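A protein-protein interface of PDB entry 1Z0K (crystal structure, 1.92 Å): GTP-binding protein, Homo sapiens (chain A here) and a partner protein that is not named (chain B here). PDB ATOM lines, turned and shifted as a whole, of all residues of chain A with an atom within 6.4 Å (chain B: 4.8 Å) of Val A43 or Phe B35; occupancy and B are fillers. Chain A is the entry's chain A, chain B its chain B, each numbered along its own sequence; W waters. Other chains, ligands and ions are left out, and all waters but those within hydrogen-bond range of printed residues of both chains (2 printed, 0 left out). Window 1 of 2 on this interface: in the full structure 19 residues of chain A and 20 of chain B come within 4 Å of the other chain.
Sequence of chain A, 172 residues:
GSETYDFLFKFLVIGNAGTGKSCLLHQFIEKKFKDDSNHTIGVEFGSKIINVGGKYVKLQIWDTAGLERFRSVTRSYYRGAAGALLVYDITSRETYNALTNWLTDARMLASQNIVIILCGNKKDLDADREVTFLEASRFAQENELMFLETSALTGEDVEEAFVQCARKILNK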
ATOM      1  N   THR A  40       7.352 -34.060 -11.064  1.00  0.00           N
ATOM      2  CA  THR A  40       7.510 -33.027 -12.089  1.00  0.00           C
ATOM      3  C   THR A  40       8.777 -33.252 -12.871  1.00  0.00           C
ATOM      4  O   THR A  40       9.866 -33.458 -12.320  1.00  0.00           O
ATOM      5  CB  THR A  40       7.405 -31.576 -11.557  1.00  0.00           C
ATOM      6  OG1 THR A  40       6.019 -31.254 -11.395  1.00  0.00           O
ATOM      7  CG2 THR A  40       8.031 -30.550 -12.529  1.00  0.00           C
ATOM      8  N   ILE A  41       8.583 -33.210 -14.178  1.00  0.00           N
ATOM      9  CA  ILE A  41       9.543 -33.668 -15.130  1.00  0.00           C
ATOM     10  C   ILE A  41      10.306 -32.442 -15.643  1.00  0.00           C
ATOM     11  O   ILE A  41      10.652 -32.324 -16.822  1.00  0.00           O
ATOM     12  CB  ILE A  41       8.797 -34.575 -16.172  1.00  0.00           C
ATOM     13  CG1 ILE A  41       8.583 -35.982 -15.572  1.00  0.00           C
ATOM     14  CG2 ILE A  41       9.516 -34.680 -17.495  1.00  0.00           C
ATOM     15  CD1 ILE A  41       9.794 -36.520 -14.793  1.00  0.00           C
ATOM     16  N   GLY A  42      10.586 -31.540 -14.703  1.00  0.00           N
ATOM     17  CA  GLY A  42      11.333 -30.324 -14.977  1.00  0.00           C
ATOM     18  C   GLY A  42      10.749 -29.161 -14.203  1.00  0.00           C
ATOM     19  O   GLY A  42      11.000 -29.017 -13.000  1.00  0.00           O
ATOM     20  N   VAL A  43       9.974 -28.329 -14.898  1.00  0.00           N
ATOM     21  CA  VAL A  43       9.344 -27.144 -14.306  1.00  0.00           C
ATOM     22  C   VAL A  43       8.061 -26.830 -15.079  1.00  0.00           C
ATOM     23  O   VAL A  43       8.111 -26.560 -16.279  1.00  0.00           O
ATOM     24  CB  VAL A  43      10.296 -25.904 -14.320  1.00  0.00           C
ATOM     25  CG1 VAL A  43       9.596 -24.670 -13.750  1.00  0.00           C
ATOM     26  CG2 VAL A  43      11.593 -26.177 -13.544  1.00  0.00           C
ATOM     27  N   GLU A  44       6.923 -26.879 -14.387  1.00  0.00           N
ATOM     28  CA  GLU A  44       5.621 -26.544 -14.970  1.00  0.00           C
ATOM     29  C   GLU A  44       5.370 -25.043 -14.954  1.00  0.00           C
ATOM     30  O   GLU A  44       5.936 -24.325 -14.128  1.00  0.00           O
ATOM     31  CB  GLU A  44       4.487 -27.219 -14.202  1.00  0.00           C
ATOM     32  CG  GLU A  44       4.223 -28.654 -14.581  1.00  0.00           C
ATOM     33  CD  GLU A  44       3.004 -29.221 -13.865  1.00  0.00           C
ATOM     34  OE1 GLU A  44       3.194 -30.126 -13.026  1.00  0.00           O
ATOM     35  OE2 GLU A  44       1.862 -28.758 -14.124  1.00  0.00           O
ATOM     36  N   PHE A  45       4.492 -24.596 -15.851  1.00  0.00           N
ATOM     37  CA  PHE A  45       4.103 -23.191 -15.947  1.00  0.00           C
ATOM     38  C   PHE A  45       2.610 -22.979 -15.770  1.00  0.00           C
ATOM     39  O   PHE A  45       1.803 -23.727 -16.305  1.00  0.00           O
ATOM     40  CB  PHE A  45       4.511 -22.604 -17.303  1.00  0.00           C
ATOM     41  CG  PHE A  45       4.150 -21.155 -17.460  1.00  0.00           C
ATOM     42  CD1 PHE A  45       4.913 -20.169 -16.843  1.00  0.00           C
ATOM     43  CD2 PHE A  45       3.038 -20.774 -18.212  1.00  0.00           C
ATOM     44  CE1 PHE A  45       4.590 -18.826 -16.979  1.00  0.00           C
ATOM     45  CE2 PHE A  45       2.705 -19.431 -18.358  1.00  0.00           C
ATOM     46  CZ  PHE A  45       3.479 -18.453 -17.742  1.00  0.00           C
ATOM     47  N   ILE A  61       3.829 -18.211 -12.890  1.00  0.00           N
ATOM     48  CA  ILE A  61       4.225 -19.167 -11.858  1.00  0.00           C
ATOM     49  C   ILE A  61       5.006 -20.316 -12.464  1.00  0.00           C
ATOM     50  O   ILE A  61       4.542 -20.978 -13.387  1.00  0.00           O
ATOM     51  CB  ILE A  61       3.000 -19.719 -11.084  1.00  0.00           C
ATOM     52  CG1 ILE A  61       2.164 -18.566 -10.516  1.00  0.00           C
ATOM     53  CG2 ILE A  61       3.448 -20.653  -9.951  1.00  0.00           C
ATOM     54  CD1 ILE A  61       0.685 -18.804 -10.580  1.00  0.00           C
ATOM     55  N   TRP A  62       6.195 -20.535 -11.914  1.00  0.00           N
ATOM     56  CA  TRP A  62       7.049 -21.638 -12.301  1.00  0.00           C
ATOM     57  C   TRP A  62       7.093 -22.651 -11.165  1.00  0.00           C
ATOM     58  O   TRP A  62       7.699 -22.400 -10.117  1.00  0.00           O
ATOM     59  CB  TRP A  62       8.447 -21.132 -12.635  1.00  0.00           C
ATOM     60  CG  TRP A  62       8.446 -20.127 -13.754  1.00  0.00           C
ATOM     61  CD1 TRP A  62       8.490 -18.770 -13.636  1.00  0.00           C
ATOM     62  CD2 TRP A  62       8.382 -20.410 -15.156  1.00  0.00           C
ATOM     63  NE1 TRP A  62       8.462 -18.185 -14.881  1.00  0.00           N
ATOM     64  CE2 TRP A  62       8.404 -19.168 -15.834  1.00  0.00           C
ATOM     65  CE3 TRP A  62       8.314 -21.592 -15.909  1.00  0.00           C
ATOM     66  CZ2 TRP A  62       8.359 -19.071 -17.237  1.00  0.00           C
ATOM     67  CZ3 TRP A  62       8.270 -21.495 -17.311  1.00  0.00           C
ATOM     68  CH2 TRP A  62       8.299 -20.246 -17.954  1.00  0.00           C
ATOM     69  N   ASP A  63       6.414 -23.774 -11.387  1.00  0.00           N
ATOM     70  CA  ASP A  63       6.353 -24.890 -10.445  1.00  0.00           C
ATOM     71  C   ASP A  63       7.525 -25.830 -10.702  1.00  0.00           C
ATOM     72  O   ASP A  63       7.520 -26.610 -11.667  1.00  0.00           O
ATOM     73  CB  ASP A  63       5.018 -25.621 -10.601  1.00  0.00           C
ATOM     74  CG  ASP A  63       5.015 -26.999  -9.959  1.00  0.00           C
ATOM     75  OD1 ASP A  63       5.550 -27.149  -8.841  1.00  0.00           O
ATOM     76  OD2 ASP A  63       4.469 -27.930 -10.583  1.00  0.00           O
ATOM     77  N   THR A  64       8.529 -25.746  -9.836  1.00  0.00           N
ATOM     78  CA  THR A  64       9.808 -26.415 -10.059  1.00  0.00           C
ATOM     79  C   THR A  64       9.773 -27.880  -9.627  1.00  0.00           C
ATOM     80  O   THR A  64       8.891 -28.291  -8.878  1.00  0.00           O
ATOM     81  CB  THR A  64      10.968 -25.674  -9.341  1.00  0.00           C
ATOM     82  OG1 THR A  64      10.818 -25.782  -7.916  1.00  0.00           O
ATOM     83  CG2 THR A  64      11.020 -24.204  -9.747  1.00  0.00           C
ATOM     84  N   ALA A  65      10.729 -28.667 -10.113  1.00  0.00           N
ATOM     85  CA  ALA A  65      10.857 -30.068  -9.712  1.00  0.00           C
ATOM     86  C   ALA A  65      11.709 -30.159  -8.459  1.00  0.00           C
ATOM     87  O   ALA A  65      12.747 -29.505  -8.370  1.00  0.00           O
ATOM     88  CB  ALA A  65      11.496 -30.871 -10.821  1.00  0.00           C
ATOM     89  N   PHE A  70      16.997 -32.768 -11.271  1.00  0.00           N
ATOM     90  CA  PHE A  70      16.551 -31.503 -11.863  1.00  0.00           C
ATOM     91  C   PHE A  70      17.049 -30.256 -11.126  1.00  0.00           C
ATOM     92  O   PHE A  70      16.577 -29.145 -11.395  1.00  0.00           O
ATOM     93  CB  PHE A  70      15.022 -31.478 -11.976  1.00  0.00           C
ATOM     94  CG  PHE A  70      14.483 -32.373 -13.050  1.00  0.00           C
ATOM     95  CD1 PHE A  70      14.490 -31.966 -14.386  1.00  0.00           C
ATOM     96  CD2 PHE A  70      13.978 -33.632 -12.735  1.00  0.00           C
ATOM     97  CE1 PHE A  70      13.996 -32.800 -15.395  1.00  0.00           C
ATOM     98  CE2 PHE A  70      13.483 -34.480 -13.736  1.00  0.00           C
ATOM     99  CZ  PHE A  70      13.488 -34.062 -15.069  1.00  0.00           C
ATOM    100  N   VAL A  73      18.352 -27.494 -13.361  1.00  0.00           N
ATOM    101  CA  VAL A  73      17.269 -26.962 -14.195  1.00  0.00           C
ATOM    102  C   VAL A  73      16.332 -26.054 -13.384  1.00  0.00           C
ATOM    103  O   VAL A  73      15.973 -24.963 -13.838  1.00  0.00           O
ATOM    104  CB  VAL A  73      16.475 -28.099 -14.903  1.00  0.00           C
ATOM    105  CG1 VAL A  73      15.236 -27.554 -15.599  1.00  0.00           C
ATOM    106  CG2 VAL A  73      17.353 -28.814 -15.910  1.00  0.00           C
ATOM    107  N   THR A  74      15.952 -26.502 -12.190  1.00  0.00           N
ATOM    108  CA  THR A  74      15.055 -25.720 -11.334  1.00  0.00           C
ATOM    109  C   THR A  74      15.711 -24.425 -10.851  1.00  0.00           C
ATOM    110  O   THR A  74      15.075 -23.369 -10.843  1.00  0.00           O
ATOM    111  CB  THR A  74      14.567 -26.522 -10.118  1.00  0.00           C
ATOM    112  OG1 THR A  74      15.680 -26.846  -9.284  1.00  0.00           O
ATOM    113  CG2 THR A  74      13.864 -27.792 -10.546  1.00  0.00           C
ATOM    114  N   TYR A  77      15.663 -21.192 -12.851  1.00  0.00           N
ATOM    115  CA  TYR A  77      14.430 -20.400 -12.848  1.00  0.00           C
ATOM    116  C   TYR A  77      14.371 -19.333 -11.748  1.00  0.00           C
ATOM    117  O   TYR A  77      13.509 -18.451 -11.790  1.00  0.00           O
ATOM    118  CB  TYR A  77      13.189 -21.309 -12.792  1.00  0.00           C
ATOM    119  CG  TYR A  77      12.855 -21.918 -14.134  1.00  0.00           C
ATOM    120  CD1 TYR A  77      11.985 -21.275 -15.014  1.00  0.00           C
ATOM    121  CD2 TYR A  77      13.425 -23.125 -14.533  1.00  0.00           C
ATOM    122  CE1 TYR A  77      11.690 -21.822 -16.250  1.00  0.00           C
ATOM    123  CE2 TYR A  77      13.136 -23.682 -15.769  1.00  0.00           C
ATOM    124  CZ  TYR A  77      12.270 -23.024 -16.623  1.00  0.00           C
ATOM    125  OH  TYR A  77      11.985 -23.559 -17.854  1.00  0.00           O
ATOM    126  N   TRP B   9      -4.503 -19.999 -16.703  1.00  0.00           N
ATOM    127  CA  TRP B   9      -4.124 -20.936 -17.750  1.00  0.00           C
ATOM    128  C   TRP B   9      -3.007 -21.845 -17.259  1.00  0.00           C
ATOM    129  O   TRP B   9      -2.063 -21.393 -16.610  1.00  0.00           O
ATOM    130  CB  TRP B   9      -3.697 -20.177 -19.016  1.00  0.00           C
ATOM    131  CG  TRP B   9      -3.282 -21.065 -20.153  1.00  0.00           C
ATOM    132  CD1 TRP B   9      -4.094 -21.824 -20.942  1.00  0.00           C
ATOM    133  CD2 TRP B   9      -1.950 -21.280 -20.625  1.00  0.00           C
ATOM    134  NE1 TRP B   9      -3.348 -22.504 -21.877  1.00  0.00           N
ATOM    135  CE2 TRP B   9      -2.029 -22.186 -21.703  1.00  0.00           C
ATOM    136  CE3 TRP B   9      -0.693 -20.795 -20.239  1.00  0.00           C
ATOM    137  CZ2 TRP B   9      -0.901 -22.617 -22.402  1.00  0.00           C
ATOM    138  CZ3 TRP B   9       0.425 -21.222 -20.932  1.00  0.00           C
ATOM    139  CH2 TRP B   9       0.315 -22.125 -22.001  1.00  0.00           C
ATOM    140  N   PRO B  11      -0.979 -25.202 -18.957  1.00  0.00           N
ATOM    141  CA  PRO B  11      -0.775 -26.135 -20.061  1.00  0.00           C
ATOM    142  C   PRO B  11      -0.474 -27.547 -19.583  1.00  0.00           C
ATOM    143  O   PRO B  11       0.188 -27.722 -18.555  1.00  0.00           O
ATOM    144  CB  PRO B  11       0.446 -25.560 -20.777  1.00  0.00           C
ATOM    145  CG  PRO B  11       1.188 -24.837 -19.709  1.00  0.00           C
ATOM    146  CD  PRO B  11       0.124 -24.234 -18.853  1.00  0.00           C
ATOM    147  N   LEU B  12      -0.968 -28.534 -20.332  1.00  0.00           N
ATOM    148  CA  LEU B  12      -0.753 -29.945 -20.020  1.00  0.00           C
ATOM    149  C   LEU B  12       0.726 -30.280 -20.157  1.00  0.00           C
ATOM    150  O   LEU B  12       1.376 -29.901 -21.141  1.00  0.00           O
ATOM    151  CB  LEU B  12      -1.581 -30.851 -20.941  1.00  0.00           C
ATOM    152  CG  LEU B  12      -3.060 -30.550 -21.208  1.00  0.00           C
ATOM    153  CD1 LEU B  12      -3.562 -31.399 -22.370  1.00  0.00           C
ATOM    154  CD2 LEU B  12      -3.927 -30.760 -19.972  1.00  0.00           C
ATOM    155  N   SER B  13       1.247 -30.983 -19.154  1.00  0.00           N
ATOM    156  CA  SER B  13       2.654 -31.365 -19.093  1.00  0.00           C
ATOM    157  C   SER B  13       3.012 -32.363 -20.196  1.00  0.00           C
ATOM    158  O   SER B  13       2.983 -33.580 -19.969  1.00  0.00           O
ATOM    159  CB  SER B  13       2.999 -31.929 -17.704  1.00  0.00           C
ATOM    160  OG  SER B  13       3.734 -30.993 -16.930  1.00  0.00           O
ATOM    161  N   GLY B  14       3.338 -31.832 -21.383  1.00  0.00           N
ATOM    162  CA  GLY B  14       3.647 -32.639 -22.572  1.00  0.00           C
ATOM    163  C   GLY B  14       2.859 -33.938 -22.589  1.00  0.00           C
ATOM    164  O   GLY B  14       3.436 -35.026 -22.501  1.00  0.00           O
ATOM    165  N   GLN B  28      13.262 -30.392 -20.016  1.00  0.00           N
ATOM    166  CA  GLN B  28      12.616 -29.099 -19.756  1.00  0.00           C
ATOM    167  C   GLN B  28      12.315 -28.352 -21.055  1.00  0.00           C
ATOM    168  O   GLN B  28      11.282 -27.700 -21.166  1.00  0.00           O
ATOM    169  CB  GLN B  28      13.435 -28.224 -18.806  1.00  0.00           C
ATOM    170  CG  GLN B  28      12.687 -26.971 -18.316  1.00  0.00           C
ATOM    171  CD  GLN B  28      11.278 -27.266 -17.799  1.00  0.00           C
ATOM    172  OE1 GLN B  28      10.982 -28.379 -17.377  1.00  0.00           O
ATOM    173  NE2 GLN B  28      10.407 -26.258 -17.821  1.00  0.00           N
ATOM    174  N   ASN B  31       9.267 -29.711 -22.489  1.00  0.00           N
ATOM    175  CA  ASN B  31       8.136 -29.180 -21.733  1.00  0.00           C
ATOM    176  C   ASN B  31       7.700 -27.815 -22.259  1.00  0.00           C
ATOM    177  O   ASN B  31       6.532 -27.611 -22.559  1.00  0.00           O
ATOM    178  CB  ASN B  31       8.453 -29.081 -20.236  1.00  0.00           C
ATOM    179  CG  ASN B  31       8.500 -30.435 -19.550  1.00  0.00           C
ATOM    180  OD1 ASN B  31       7.969 -31.430 -20.052  1.00  0.00           O
ATOM    181  ND2 ASN B  31       9.126 -30.473 -18.382  1.00  0.00           N
ATOM    182  N   ILE B  32       8.658 -26.902 -22.379  1.00  0.00           N
ATOM    183  CA  ILE B  32       8.370 -25.530 -22.809  1.00  0.00           C
ATOM    184  C   ILE B  32       7.855 -25.516 -24.246  1.00  0.00           C
ATOM    185  O   ILE B  32       6.915 -24.793 -24.572  1.00  0.00           O
ATOM    186  CB  ILE B  32       9.608 -24.606 -22.626  1.00  0.00           C
ATOM    187  CG1 ILE B  32      10.034 -24.572 -21.149  1.00  0.00           C
ATOM    188  CG2 ILE B  32       9.333 -23.193 -23.157  1.00  0.00           C
ATOM    189  CD1 ILE B  32       8.940 -24.130 -20.156  1.00  0.00           C
ATOM    190  N   THR B  33       8.451 -26.350 -25.092  1.00  0.00           N
ATOM    191  CA  THR B  33       8.006 -26.484 -26.473  1.00  0.00           C
ATOM    192  C   THR B  33       6.538 -26.896 -26.543  1.00  0.00           C
ATOM    193  O   THR B  33       5.760 -26.357 -27.347  1.00  0.00           O
ATOM    194  CB  THR B  33       8.906 -27.468 -27.228  1.00  0.00           C
ATOM    195  OG1 THR B  33      10.219 -26.900 -27.302  1.00  0.00           O
ATOM    196  CG2 THR B  33       8.385 -27.705 -28.635  1.00  0.00           C
ATOM    197  N   SER B  34       6.159 -27.836 -25.681  1.00  0.00           N
ATOM    198  CA  SER B  34       4.764 -28.254 -25.559  1.00  0.00           C
ATOM    199  C   SER B  34       3.864 -27.126 -25.061  1.00  0.00           C
ATOM    200  O   SER B  34       2.774 -26.928 -25.600  1.00  0.00           O
ATOM    201  CB  SER B  34       4.631 -29.483 -24.661  1.00  0.00           C
ATOM    202  OG  SER B  34       3.266 -29.822 -24.487  1.00  0.00           O
ATOM    203  N   PHE B  35       4.311 -26.398 -24.033  1.00  0.00           N
ATOM    204  CA  PHE B  35       3.528 -25.278 -23.496  1.00  0.00           C
ATOM    205  C   PHE B  35       3.325 -24.183 -24.558  1.00  0.00           C
ATOM    206  O   PHE B  35       2.244 -23.605 -24.635  1.00  0.00           O
ATOM    207  CB  PHE B  35       4.176 -24.644 -22.250  1.00  0.00           C
ATOM    208  CG  PHE B  35       4.433 -25.601 -21.100  1.00  0.00           C
ATOM    209  CD1 PHE B  35       3.775 -26.827 -21.001  1.00  0.00           C
ATOM    210  CD2 PHE B  35       5.326 -25.239 -20.092  1.00  0.00           C
ATOM    211  CE1 PHE B  35       4.025 -27.678 -19.933  1.00  0.00           C
ATOM    212  CE2 PHE B  35       5.577 -26.091 -19.003  1.00  0.00           C
ATOM    213  CZ  PHE B  35       4.929 -27.312 -18.935  1.00  0.00           C
ATOM    214  N   ILE B  36       4.364 -23.907 -25.355  1.00  0.00           N
ATOM    215  CA  ILE B  36       4.299 -22.905 -26.442  1.00  0.00           C
ATOM    216  C   ILE B  36       3.256 -23.283 -27.494  1.00  0.00           C
ATOM    217  O   ILE B  36       2.482 -22.430 -27.936  1.00  0.00           O
ATOM    218  CB  ILE B  36       5.672 -22.675 -27.130  1.00  0.00           C
ATOM    219  CG1 ILE B  36       6.651 -21.999 -26.167  1.00  0.00           C
ATOM    220  CG2 ILE B  36       5.517 -21.808 -28.419  1.00  0.00           C
ATOM    221  CD1 ILE B  36       8.068 -21.927 -26.677  1.00  0.00           C
ATOM    222  N   ARG B  37       3.249 -24.556 -27.887  1.00  0.00           N
ATOM    223  CA  ARG B  37       2.261 -25.098 -28.824  1.00  0.00           C
ATOM    224  C   ARG B  37       0.840 -24.876 -28.298  1.00  0.00           C
ATOM    225  O   ARG B  37      -0.047 -24.470 -29.047  1.00  0.00           O
ATOM    226  CB  ARG B  37       2.553 -26.585 -29.082  1.00  0.00           C
ATOM    227  CG  ARG B  37       1.565 -27.317 -29.986  1.00  0.00           C
ATOM    228  CD  ARG B  37       1.870 -28.825 -30.049  1.00  0.00           C
ATOM    229  NE  ARG B  37       2.150 -29.416 -28.732  1.00  0.00           N
ATOM    230  CZ  ARG B  37       1.227 -29.859 -27.880  1.00  0.00           C
ATOM    231  NH1 ARG B  37      -0.062 -29.796 -28.188  1.00  0.00           N
ATOM    232  NH2 ARG B  37       1.593 -30.370 -26.711  1.00  0.00           N
ATOM    233  N   GLN B  38       0.635 -25.116 -27.004  1.00  0.00           N
ATOM    234  CA  GLN B  38      -0.679 -24.922 -26.385  1.00  0.00           C
ATOM    235  C   GLN B  38      -1.029 -23.443 -26.224  1.00  0.00           C
ATOM    236  O   GLN B  38      -2.181 -23.053 -26.432  1.00  0.00           O
ATOM    237  CB  GLN B  38      -0.771 -25.650 -25.044  1.00  0.00           C
ATOM    238  CG  GLN B  38      -0.499 -27.163 -25.122  1.00  0.00           C
ATOM    239  CD  GLN B  38      -0.402 -27.808 -23.748  1.00  0.00           C
ATOM    240  OE1 GLN B  38      -1.362 -27.785 -22.968  1.00  0.00           O
ATOM    241  NE2 GLN B  38       0.760 -28.385 -23.444  1.00  0.00           N
ATOM    242  N   ALA B  39      -0.048 -22.617 -25.863  1.00  0.00           N
ATOM    243  CA  ALA B  39      -0.294 -21.175 -25.742  1.00  0.00           C
ATOM    244  C   ALA B  39      -0.654 -20.568 -27.106  1.00  0.00           C
ATOM    245  O   ALA B  39      -1.606 -19.785 -27.211  1.00  0.00           O
ATOM    246  CB  ALA B  39       0.900 -20.465 -25.118  1.00  0.00           C
ATOM    247  N   LEU B  51       6.998 -17.779 -22.735  1.00  0.00           N
ATOM    248  CA  LEU B  51       7.539 -19.128 -22.855  1.00  0.00           C
ATOM    249  C   LEU B  51       8.635 -19.204 -23.899  1.00  0.00           C
ATOM    250  O   LEU B  51       9.597 -19.952 -23.735  1.00  0.00           O
ATOM    251  CB  LEU B  51       6.426 -20.132 -23.152  1.00  0.00           C
ATOM    252  CG  LEU B  51       5.416 -20.357 -22.023  1.00  0.00           C
ATOM    253  CD1 LEU B  51       4.140 -20.951 -22.574  1.00  0.00           C
ATOM    254  CD2 LEU B  51       6.012 -21.233 -20.912  1.00  0.00           C
HETATM  255  O   HOH W   1       2.469 -26.316 -16.944  1.00  0.00           O
HETATM  256  O   HOH W   2       0.817 -29.256 -16.517  1.00  0.00           O
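Water W2 lies within hydrogen-bond range of the backbone carbonyl oxygen (O) of Pro B11, the side-chain carboxylate (OE2) of Glu A44 and the backbone NH (N) of Ser B13. Water W1 bridges O of Phe A45 (2.7 Å) and O of Pro B11 (3.1 Å).
Gly A42 touches Gln B28 (CA to OE1, 3.1 Å). Val A43 touches Phe B35. Glu A44 touches Ser B13. Phe A45 touches Trp B9. Phe A45 touches Pro B11 (O to CD, 3.1 Å). Phe A45 touches Leu B51 (CG to CD2, 3.9 Å). CD1 of Ile B32 touches CZ3 of Trp A62, 3.9 Å away. CH2 of Trp A62 touches CD2 of Leu B51 (3.9 Å). CG1 of Val A73 touches CB of Gln B28, at 3.7 Å. OH of Tyr A77 touches CD1 of Ile B32 (3.9 Å).
The side-chain amide nitrogen (ND2) of Asn B31 lies within hydrogen-bond range of the backbone carbonyl oxygen (O) of Ile A41 (2.9 Å). The backbone NH of Val A43 is in hydrogen-bond range of the side-chain amide oxygen of Gln B28, at 2.7 Å. OH of Tyr A77 sits at hydrogen-bond distance from NE2 of Gln B28 (3.1 Å).
Of the 16 printed residues of chain B, 8 touch a printed residue of chain A. Along chain B the printed residues that touch a printed residue of chain A span positions 9 to 51. Printed residues of chain A that touch a printed residue of chain B: Ile A41, Gly A42, Val A43, Glu A44, Phe A45, Trp A62, Val A73 and Tyr A77. Among the printed residues, 15 pairs touch across the chains.
The side-chain hydroxyl of Thr A40 sits close to the side-chain carboxylate of Glu A44. The backbone NH (N) of Ala A65 lies close to the backbone carbonyl oxygen (O) of Gly A42. The backbone carbonyl oxygen (O) of Asp A63 lies within hydrogen-bond range of the backbone NH (N) of Glu A44 (2.8 Å). ND2 of Asn B31 sits at hydrogen-bond distance from OE1 of Gln B28, 3.0 Å away.
Of chain B, only Gln B28 (2.7 Å) and Phe B35 (3.7 Å) come within 4 Å of Val A43. Phe B35 touches just these residues of chain A: Val A43 and Phe A45. Of the printed residues of chain B, Val A73 touches Gln B28 (3.7 Å). Printed residues of chain B within 4 Å of Gly A42: Gln B28. Of the printed residues of chain B, Phe A45 touches Trp B9, Pro B11, Phe B35 and Leu B51. Of the printed residues of chain A, Ser B13 touches Glu A44.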
